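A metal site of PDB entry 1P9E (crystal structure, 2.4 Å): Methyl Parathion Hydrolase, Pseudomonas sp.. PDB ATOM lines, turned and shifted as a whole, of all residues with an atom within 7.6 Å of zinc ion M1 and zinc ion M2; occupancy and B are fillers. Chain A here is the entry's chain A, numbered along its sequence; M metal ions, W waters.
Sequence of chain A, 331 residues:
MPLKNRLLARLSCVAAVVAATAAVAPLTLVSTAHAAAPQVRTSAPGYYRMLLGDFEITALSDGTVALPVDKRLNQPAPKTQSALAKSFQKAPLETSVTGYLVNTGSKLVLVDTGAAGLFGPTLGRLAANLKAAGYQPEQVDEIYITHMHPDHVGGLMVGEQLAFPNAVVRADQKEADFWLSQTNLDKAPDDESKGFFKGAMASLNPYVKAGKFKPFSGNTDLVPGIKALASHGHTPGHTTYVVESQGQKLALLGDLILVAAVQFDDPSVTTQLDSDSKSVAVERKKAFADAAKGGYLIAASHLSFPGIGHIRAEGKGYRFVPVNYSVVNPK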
ATOM      1  N   LEU A  67      10.640  14.784 -31.846  1.00  0.00           N
ATOM      2  CA  LEU A  67      11.782  15.233 -32.625  1.00  0.00           C
ATOM      3  C   LEU A  67      12.279  14.182 -33.615  1.00  0.00           C
ATOM      4  O   LEU A  67      12.262  12.981 -33.331  1.00  0.00           O
ATOM      5  CB  LEU A  67      12.937  15.607 -31.685  1.00  0.00           C
ATOM      6  CG  LEU A  67      12.597  16.696 -30.663  1.00  0.00           C
ATOM      7  CD1 LEU A  67      13.767  16.866 -29.677  1.00  0.00           C
ATOM      8  CD2 LEU A  67      12.263  17.999 -31.391  1.00  0.00           C
ATOM      9  N   SER A  96      11.330  14.663 -23.735  1.00  0.00           N
ATOM     10  CA  SER A  96      10.964  15.522 -22.634  1.00  0.00           C
ATOM     11  C   SER A  96      11.891  16.748 -22.633  1.00  0.00           C
ATOM     12  O   SER A  96      13.022  16.683 -23.136  1.00  0.00           O
ATOM     13  CB  SER A  96      11.040  14.746 -21.309  1.00  0.00           C
ATOM     14  OG  SER A  96      12.367  14.331 -21.056  1.00  0.00           O
ATOM     15  N   VAL A  97      11.389  17.858 -22.108  1.00  0.00           N
ATOM     16  CA  VAL A  97      12.140  19.111 -22.022  1.00  0.00           C
ATOM     17  C   VAL A  97      12.091  19.432 -20.536  1.00  0.00           C
ATOM     18  O   VAL A  97      11.007  19.653 -19.994  1.00  0.00           O
ATOM     19  CB  VAL A  97      11.453  20.219 -22.821  1.00  0.00           C
ATOM     20  CG1 VAL A  97      12.161  21.543 -22.588  1.00  0.00           C
ATOM     21  CG2 VAL A  97      11.445  19.853 -24.310  1.00  0.00           C
ATOM     22  N   THR A  98      13.256  19.463 -19.889  1.00  0.00           N
ATOM     23  CA  THR A  98      13.300  19.658 -18.442  1.00  0.00           C
ATOM     24  C   THR A  98      14.202  20.750 -17.839  1.00  0.00           C
ATOM     25  O   THR A  98      15.240  21.127 -18.404  1.00  0.00           O
ATOM     26  CB  THR A  98      13.662  18.297 -17.802  1.00  0.00           C
ATOM     27  OG1 THR A  98      12.834  17.276 -18.385  1.00  0.00           O
ATOM     28  CG2 THR A  98      13.416  18.309 -16.301  1.00  0.00           C
ATOM     29  N   ASP A 112      17.656  26.389 -16.086  1.00  0.00           N
ATOM     30  CA  ASP A 112      16.919  26.355 -17.334  1.00  0.00           C
ATOM     31  C   ASP A 112      15.460  26.602 -17.014  1.00  0.00           C
ATOM     32  O   ASP A 112      14.979  26.260 -15.921  1.00  0.00           O
ATOM     33  CB  ASP A 112      17.185  25.038 -18.063  1.00  0.00           C
ATOM     34  CG  ASP A 112      18.549  25.055 -18.775  1.00  0.00           C
ATOM     35  OD1 ASP A 112      18.946  24.043 -19.379  1.00  0.00           O
ATOM     36  OD2 ASP A 112      19.235  26.114 -18.711  1.00  0.00           O
ATOM     37  N   THR A 146      21.985  26.817 -19.040  1.00  0.00           N
ATOM     38  CA  THR A 146      23.012  25.927 -19.572  1.00  0.00           C
ATOM     39  C   THR A 146      23.403  26.532 -20.934  1.00  0.00           C
ATOM     40  O   THR A 146      24.587  26.700 -21.238  1.00  0.00           O
ATOM     41  CB  THR A 146      22.483  24.463 -19.752  1.00  0.00           C
ATOM     42  OG1 THR A 146      21.280  24.463 -20.522  1.00  0.00           O
ATOM     43  CG2 THR A 146      22.184  23.834 -18.390  1.00  0.00           C
ATOM     44  N   HIS A 147      22.398  26.853 -21.752  1.00  0.00           N
ATOM     45  CA  HIS A 147      22.636  27.461 -23.052  1.00  0.00           C
ATOM     46  C   HIS A 147      21.371  28.192 -23.473  1.00  0.00           C
ATOM     47  O   HIS A 147      20.276  27.916 -22.945  1.00  0.00           O
ATOM     48  CB  HIS A 147      23.074  26.431 -24.111  1.00  0.00           C
ATOM     49  CG  HIS A 147      22.076  25.349 -24.363  1.00  0.00           C
ATOM     50  ND1 HIS A 147      21.641  24.480 -23.387  1.00  0.00           N
ATOM     51  CD2 HIS A 147      21.431  24.975 -25.509  1.00  0.00           C
ATOM     52  CE1 HIS A 147      20.789  23.614 -23.914  1.00  0.00           C
ATOM     53  NE2 HIS A 147      20.650  23.892 -25.194  1.00  0.00           N
ATOM     54  N   MET A 148      21.508  29.121 -24.409  1.00  0.00           N
ATOM     55  CA  MET A 148      20.357  29.922 -24.829  1.00  0.00           C
ATOM     56  C   MET A 148      19.481  29.432 -25.963  1.00  0.00           C
ATOM     57  O   MET A 148      19.061  30.231 -26.801  1.00  0.00           O
ATOM     58  CB  MET A 148      20.820  31.344 -25.136  1.00  0.00           C
ATOM     59  CG  MET A 148      21.311  32.087 -23.906  1.00  0.00           C
ATOM     60  SD  MET A 148      21.848  33.753 -24.293  1.00  0.00           S
ATOM     61  CE  MET A 148      22.997  34.081 -22.870  1.00  0.00           C
ATOM     62  N   HIS A 149      19.193  28.139 -26.003  1.00  0.00           N
ATOM     63  CA  HIS A 149      18.291  27.651 -27.026  1.00  0.00           C
ATOM     64  C   HIS A 149      16.880  28.007 -26.605  1.00  0.00           C
ATOM     65  O   HIS A 149      16.619  28.254 -25.423  1.00  0.00           O
ATOM     66  CB  HIS A 149      18.459  26.150 -27.218  1.00  0.00           C
ATOM     67  CG  HIS A 149      19.455  25.798 -28.271  1.00  0.00           C
ATOM     68  ND1 HIS A 149      19.888  24.504 -28.493  1.00  0.00           N
ATOM     69  CD2 HIS A 149      20.085  26.569 -29.193  1.00  0.00           C
ATOM     70  CE1 HIS A 149      20.754  24.503 -29.497  1.00  0.00           C
ATOM     71  NE2 HIS A 149      20.886  25.739 -29.937  1.00  0.00           N
ATOM     72  N   PRO A 150      15.945  28.015 -27.555  1.00  0.00           N
ATOM     73  CA  PRO A 150      14.550  28.356 -27.252  1.00  0.00           C
ATOM     74  C   PRO A 150      13.970  27.573 -26.078  1.00  0.00           C
ATOM     75  O   PRO A 150      13.305  28.153 -25.210  1.00  0.00           O
ATOM     76  CB  PRO A 150      13.817  28.042 -28.560  1.00  0.00           C
ATOM     77  CG  PRO A 150      14.892  28.087 -29.603  1.00  0.00           C
ATOM     78  CD  PRO A 150      16.077  27.470 -28.924  1.00  0.00           C
ATOM     79  N   ASP A 151      14.223  26.269 -26.062  1.00  0.00           N
ATOM     80  CA  ASP A 151      13.687  25.385 -25.027  1.00  0.00           C
ATOM     81  C   ASP A 151      14.418  25.453 -23.675  1.00  0.00           C
ATOM     82  O   ASP A 151      14.249  24.588 -22.807  1.00  0.00           O
ATOM     83  CB  ASP A 151      13.643  23.941 -25.542  1.00  0.00           C
ATOM     84  CG  ASP A 151      15.006  23.443 -25.987  1.00  0.00           C
ATOM     85  OD1 ASP A 151      15.685  24.169 -26.763  1.00  0.00           O
ATOM     86  OD2 ASP A 151      15.398  22.325 -25.552  1.00  0.00           O
ATOM     87  N   HIS A 152      15.231  26.495 -23.497  1.00  0.00           N
ATOM     88  CA  HIS A 152      15.918  26.661 -22.241  1.00  0.00           C
ATOM     89  C   HIS A 152      15.734  28.077 -21.734  1.00  0.00           C
ATOM     90  O   HIS A 152      15.715  28.307 -20.524  1.00  0.00           O
ATOM     91  CB  HIS A 152      17.389  26.303 -22.413  1.00  0.00           C
ATOM     92  CG  HIS A 152      17.618  24.865 -22.759  1.00  0.00           C
ATOM     93  ND1 HIS A 152      17.994  23.931 -21.822  1.00  0.00           N
ATOM     94  CD2 HIS A 152      17.440  24.190 -23.923  1.00  0.00           C
ATOM     95  CE1 HIS A 152      18.032  22.738 -22.387  1.00  0.00           C
ATOM     96  NE2 HIS A 152      17.705  22.859 -23.665  1.00  0.00           N
ATOM     97  N   TRP A 179      24.642  34.792 -28.899  1.00  0.00           N
ATOM     98  CA  TRP A 179      23.208  34.910 -29.165  1.00  0.00           C
ATOM     99  C   TRP A 179      22.613  36.324 -29.133  1.00  0.00           C
ATOM    100  O   TRP A 179      21.677  36.624 -29.881  1.00  0.00           O
ATOM    101  CB  TRP A 179      22.413  34.028 -28.177  1.00  0.00           C
ATOM    102  CG  TRP A 179      22.648  32.560 -28.382  1.00  0.00           C
ATOM    103  CD1 TRP A 179      23.333  31.714 -27.560  1.00  0.00           C
ATOM    104  CD2 TRP A 179      22.185  31.778 -29.479  1.00  0.00           C
ATOM    105  NE1 TRP A 179      23.335  30.447 -28.080  1.00  0.00           N
ATOM    106  CE2 TRP A 179      22.632  30.451 -29.261  1.00  0.00           C
ATOM    107  CE3 TRP A 179      21.428  32.054 -30.621  1.00  0.00           C
ATOM    108  CZ2 TRP A 179      22.351  29.408 -30.156  1.00  0.00           C
ATOM    109  CZ3 TRP A 179      21.157  31.012 -31.515  1.00  0.00           C
ATOM    110  CH2 TRP A 179      21.622  29.702 -31.270  1.00  0.00           C
ATOM    111  N   PHE A 196      16.062  31.837 -33.438  1.00  0.00           N
ATOM    112  CA  PHE A 196      16.807  31.435 -32.259  1.00  0.00           C
ATOM    113  C   PHE A 196      17.467  32.689 -31.686  1.00  0.00           C
ATOM    114  O   PHE A 196      17.396  32.934 -30.482  1.00  0.00           O
ATOM    115  CB  PHE A 196      17.879  30.401 -32.623  1.00  0.00           C
ATOM    116  CG  PHE A 196      17.342  29.008 -32.758  1.00  0.00           C
ATOM    117  CD1 PHE A 196      16.275  28.733 -33.602  1.00  0.00           C
ATOM    118  CD2 PHE A 196      17.906  27.969 -32.023  1.00  0.00           C
ATOM    119  CE1 PHE A 196      15.770  27.447 -33.728  1.00  0.00           C
ATOM    120  CE2 PHE A 196      17.400  26.675 -32.137  1.00  0.00           C
ATOM    121  CZ  PHE A 196      16.323  26.410 -32.984  1.00  0.00           C
ATOM    122  N   HIS A 234      28.089  22.153 -27.606  1.00  0.00           N
ATOM    123  CA  HIS A 234      26.717  22.113 -28.089  1.00  0.00           C
ATOM    124  C   HIS A 234      26.478  23.518 -28.619  1.00  0.00           C
ATOM    125  O   HIS A 234      25.854  23.712 -29.664  1.00  0.00           O
ATOM    126  CB  HIS A 234      25.721  21.784 -26.958  1.00  0.00           C
ATOM    127  CG  HIS A 234      24.283  21.793 -27.385  1.00  0.00           C
ATOM    128  ND1 HIS A 234      23.797  21.005 -28.410  1.00  0.00           N
ATOM    129  CD2 HIS A 234      23.213  22.509 -26.930  1.00  0.00           C
ATOM    130  CE1 HIS A 234      22.500  21.228 -28.567  1.00  0.00           C
ATOM    131  NE2 HIS A 234      22.120  22.140 -27.684  1.00  0.00           N
ATOM    132  N   THR A 235      26.981  24.494 -27.861  1.00  0.00           N
ATOM    133  CA  THR A 235      26.903  25.918 -28.221  1.00  0.00           C
ATOM    134  C   THR A 235      28.219  26.525 -27.712  1.00  0.00           C
ATOM    135  O   THR A 235      28.893  25.921 -26.861  1.00  0.00           O
ATOM    136  CB  THR A 235      25.677  26.617 -27.607  1.00  0.00           C
ATOM    137  OG1 THR A 235      25.726  26.499 -26.183  1.00  0.00           O
ATOM    138  CG2 THR A 235      24.393  25.991 -28.120  1.00  0.00           C
ATOM    139  N   HIS A 238      28.102  26.667 -23.800  1.00  0.00           N
ATOM    140  CA  HIS A 238      27.256  25.696 -23.103  1.00  0.00           C
ATOM    141  C   HIS A 238      27.870  25.450 -21.740  1.00  0.00           C
ATOM    142  O   HIS A 238      29.085  25.254 -21.614  1.00  0.00           O
ATOM    143  CB  HIS A 238      27.143  24.380 -23.897  1.00  0.00           C
ATOM    144  CG  HIS A 238      26.241  23.374 -23.247  1.00  0.00           C
ATOM    145  ND1 HIS A 238      26.701  22.348 -22.470  1.00  0.00           N
ATOM    146  CD2 HIS A 238      24.883  23.282 -23.236  1.00  0.00           C
ATOM    147  CE1 HIS A 238      25.682  21.654 -21.998  1.00  0.00           C
ATOM    148  NE2 HIS A 238      24.563  22.205 -22.443  1.00  0.00           N
ATOM    149  N   GLY A 254      22.574  19.967 -18.939  1.00  0.00           N
ATOM    150  CA  GLY A 254      21.989  20.706 -20.040  1.00  0.00           C
ATOM    151  C   GLY A 254      21.711  19.808 -21.254  1.00  0.00           C
ATOM    152  O   GLY A 254      21.055  18.771 -21.136  1.00  0.00           O
ATOM    153  N   ASP A 255      22.191  20.203 -22.430  1.00  0.00           N
ATOM    154  CA  ASP A 255      21.983  19.422 -23.645  1.00  0.00           C
ATOM    155  C   ASP A 255      23.326  18.742 -23.979  1.00  0.00           C
ATOM    156  O   ASP A 255      23.628  18.479 -25.154  1.00  0.00           O
ATOM    157  CB  ASP A 255      21.540  20.328 -24.826  1.00  0.00           C
ATOM    158  CG  ASP A 255      20.044  20.692 -24.801  1.00  0.00           C
ATOM    159  OD1 ASP A 255      19.357  20.342 -23.811  1.00  0.00           O
ATOM    160  OD2 ASP A 255      19.542  21.332 -25.772  1.00  0.00           O
ATOM    161  N   LEU A 256      24.139  18.460 -22.975  1.00  0.00           N
ATOM    162  CA  LEU A 256      25.427  17.818 -23.259  1.00  0.00           C
ATOM    163  C   LEU A 256      25.193  16.470 -23.971  1.00  0.00           C
ATOM    164  O   LEU A 256      26.067  15.967 -24.700  1.00  0.00           O
ATOM    165  CB  LEU A 256      26.233  17.599 -21.972  1.00  0.00           C
ATOM    166  CG  LEU A 256      27.720  17.999 -22.023  1.00  0.00           C
ATOM    167  CD1 LEU A 256      28.470  17.213 -20.953  1.00  0.00           C
ATOM    168  CD2 LEU A 256      28.304  17.700 -23.399  1.00  0.00           C
ATOM    169  N   ILE A 257      24.004  15.887 -23.729  1.00  0.00           N
ATOM    170  CA  ILE A 257      23.577  14.654 -24.374  1.00  0.00           C
ATOM    171  C   ILE A 257      22.122  14.853 -24.772  1.00  0.00           C
ATOM    172  O   ILE A 257      21.325  15.367 -23.979  1.00  0.00           O
ATOM    173  CB  ILE A 257      23.718  13.397 -23.473  1.00  0.00           C
ATOM    174  CG1 ILE A 257      22.987  12.221 -24.139  1.00  0.00           C
ATOM    175  CG2 ILE A 257      23.177  13.661 -22.087  1.00  0.00           C
ATOM    176  CD1 ILE A 257      23.386  10.849 -23.649  1.00  0.00           C
ATOM    177  N   LEU A 258      21.793  14.472 -26.000  1.00  0.00           N
ATOM    178  CA  LEU A 258      20.446  14.662 -26.564  1.00  0.00           C
ATOM    179  C   LEU A 258      19.572  13.408 -26.801  1.00  0.00           C
ATOM    180  O   LEU A 258      18.336  13.504 -26.722  1.00  0.00           O
ATOM    181  CB  LEU A 258      20.564  15.408 -27.901  1.00  0.00           C
ATOM    182  CG  LEU A 258      21.342  16.723 -27.868  1.00  0.00           C
ATOM    183  CD1 LEU A 258      21.677  17.178 -29.282  1.00  0.00           C
ATOM    184  CD2 LEU A 258      20.504  17.792 -27.149  1.00  0.00           C
ATOM    185  N   LEU A 273      23.051  19.686 -34.636  1.00  0.00           N
ATOM    186  CA  LEU A 273      22.607  20.766 -33.762  1.00  0.00           C
ATOM    187  C   LEU A 273      23.753  21.305 -32.910  1.00  0.00           C
ATOM    188  O   LEU A 273      23.604  22.333 -32.264  1.00  0.00           O
ATOM    189  CB  LEU A 273      21.482  20.276 -32.850  1.00  0.00           C
ATOM    190  CG  LEU A 273      20.272  19.740 -33.625  1.00  0.00           C
ATOM    191  CD1 LEU A 273      19.449  18.785 -32.776  1.00  0.00           C
ATOM    192  CD2 LEU A 273      19.444  20.936 -34.082  1.00  0.00           C
ATOM    193  N   ASP A 274      24.893  20.601 -32.922  1.00  0.00           N
ATOM    194  CA  ASP A 274      26.064  20.992 -32.138  1.00  0.00           C
ATOM    195  C   ASP A 274      26.997  21.913 -32.901  1.00  0.00           C
ATOM    196  O   ASP A 274      27.203  21.739 -34.102  1.00  0.00           O
ATOM    197  CB  ASP A 274      26.857  19.750 -31.694  1.00  0.00           C
ATOM    198  CG  ASP A 274      26.030  18.826 -30.842  1.00  0.00           C
ATOM    199  OD1 ASP A 274      25.680  19.213 -29.697  1.00  0.00           O
ATOM    200  OD2 ASP A 274      25.737  17.704 -31.309  1.00  0.00           O
ATOM    201  N   SER A 301      18.484  17.835 -19.842  1.00  0.00           N
ATOM    202  CA  SER A 301      17.184  18.354 -20.240  1.00  0.00           C
ATOM    203  C   SER A 301      16.329  17.444 -21.095  1.00  0.00           C
ATOM    204  O   SER A 301      15.102  17.617 -21.135  1.00  0.00           O
ATOM    205  CB  SER A 301      17.371  19.683 -20.963  1.00  0.00           C
ATOM    206  OG  SER A 301      18.289  20.521 -20.262  1.00  0.00           O
ATOM    207  N   HIS A 302      16.938  16.468 -21.787  1.00  0.00           N
ATOM    208  CA  HIS A 302      16.149  15.618 -22.673  1.00  0.00           C
ATOM    209  C   HIS A 302      16.158  14.119 -22.444  1.00  0.00           C
ATOM    210  O   HIS A 302      15.773  13.375 -23.349  1.00  0.00           O
ATOM    211  CB  HIS A 302      16.506  15.944 -24.119  1.00  0.00           C
ATOM    212  CG  HIS A 302      16.343  17.402 -24.440  1.00  0.00           C
ATOM    213  ND1 HIS A 302      15.134  18.055 -24.359  1.00  0.00           N
ATOM    214  CD2 HIS A 302      17.255  18.351 -24.749  1.00  0.00           C
ATOM    215  CE1 HIS A 302      15.313  19.348 -24.603  1.00  0.00           C
ATOM    216  NE2 HIS A 302      16.592  19.549 -24.837  1.00  0.00           N
HETATM  217 ZN    ZN M   1      20.211  22.839 -27.316  1.00  0.00          ZN
HETATM  218 ZN    ZN M   2      17.388  21.525 -25.297  1.00  0.00          ZN
HETATM  219  O   HOH W   1      19.531  21.224 -29.083  1.00  0.00           O
HETATM  220  O   HOH W   2      18.078  22.721 -26.997  1.00  0.00           O
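A ring nitrogen (ND1) of His 234 lies within hydrogen-bond range of the side-chain carboxylate (OD1) of Asp 274. A ring nitrogen (ND1) of His 152 sits at hydrogen-bond distance from the side-chain carboxylate of Asp 112. A ring nitrogen (ND1) of His 302 is in hydrogen-bond range of the backbone carbonyl oxygen (O) of Ser 96, 2.8 Å away. N of Asp 255 sits at hydrogen-bond distance from NE2 of His 238 (3.1 Å). A ring nitrogen (ND1) of His 147 lies within hydrogen-bond range of the side-chain hydroxyl (OG1) of Thr 146, at 2.9 Å.
Within 4 Å of zinc ion M1: His 147, His 149, His 234 and Asp 255. Along chain A the residues within 4 Å of zinc ion M1 span positions 147 to 255.
Four residues have an atom within 4 Å of zinc ion M2: Asp 151, His 152, Asp 255 and His 302.
Zinc ion M1 is bound by a ring nitrogen (ND1) of His 149, a ring nitrogen (NE2) of His 234, water W2, the side-chain carboxylate (OD2) of Asp 255, a ring nitrogen (NE2) of His 147 and water W1.
NE2 of His 152 binds zinc ion M2 (2.1 Å). Zinc ion M2 is bound by OD2 of Asp 151 (2.2 Å). A ring nitrogen (NE2) of His 302 binds zinc ion M2, 2.2 Å away. Water W2 binds zinc ion M2, at 2.2 Å. The side-chain carboxylate (OD2) of Asp 255 binds zinc ion M2, 2.2 Å away. Slightly farther from zinc ion M2 lies the side-chain carboxylate (OD1) of Asp 255 (2.7 Å).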
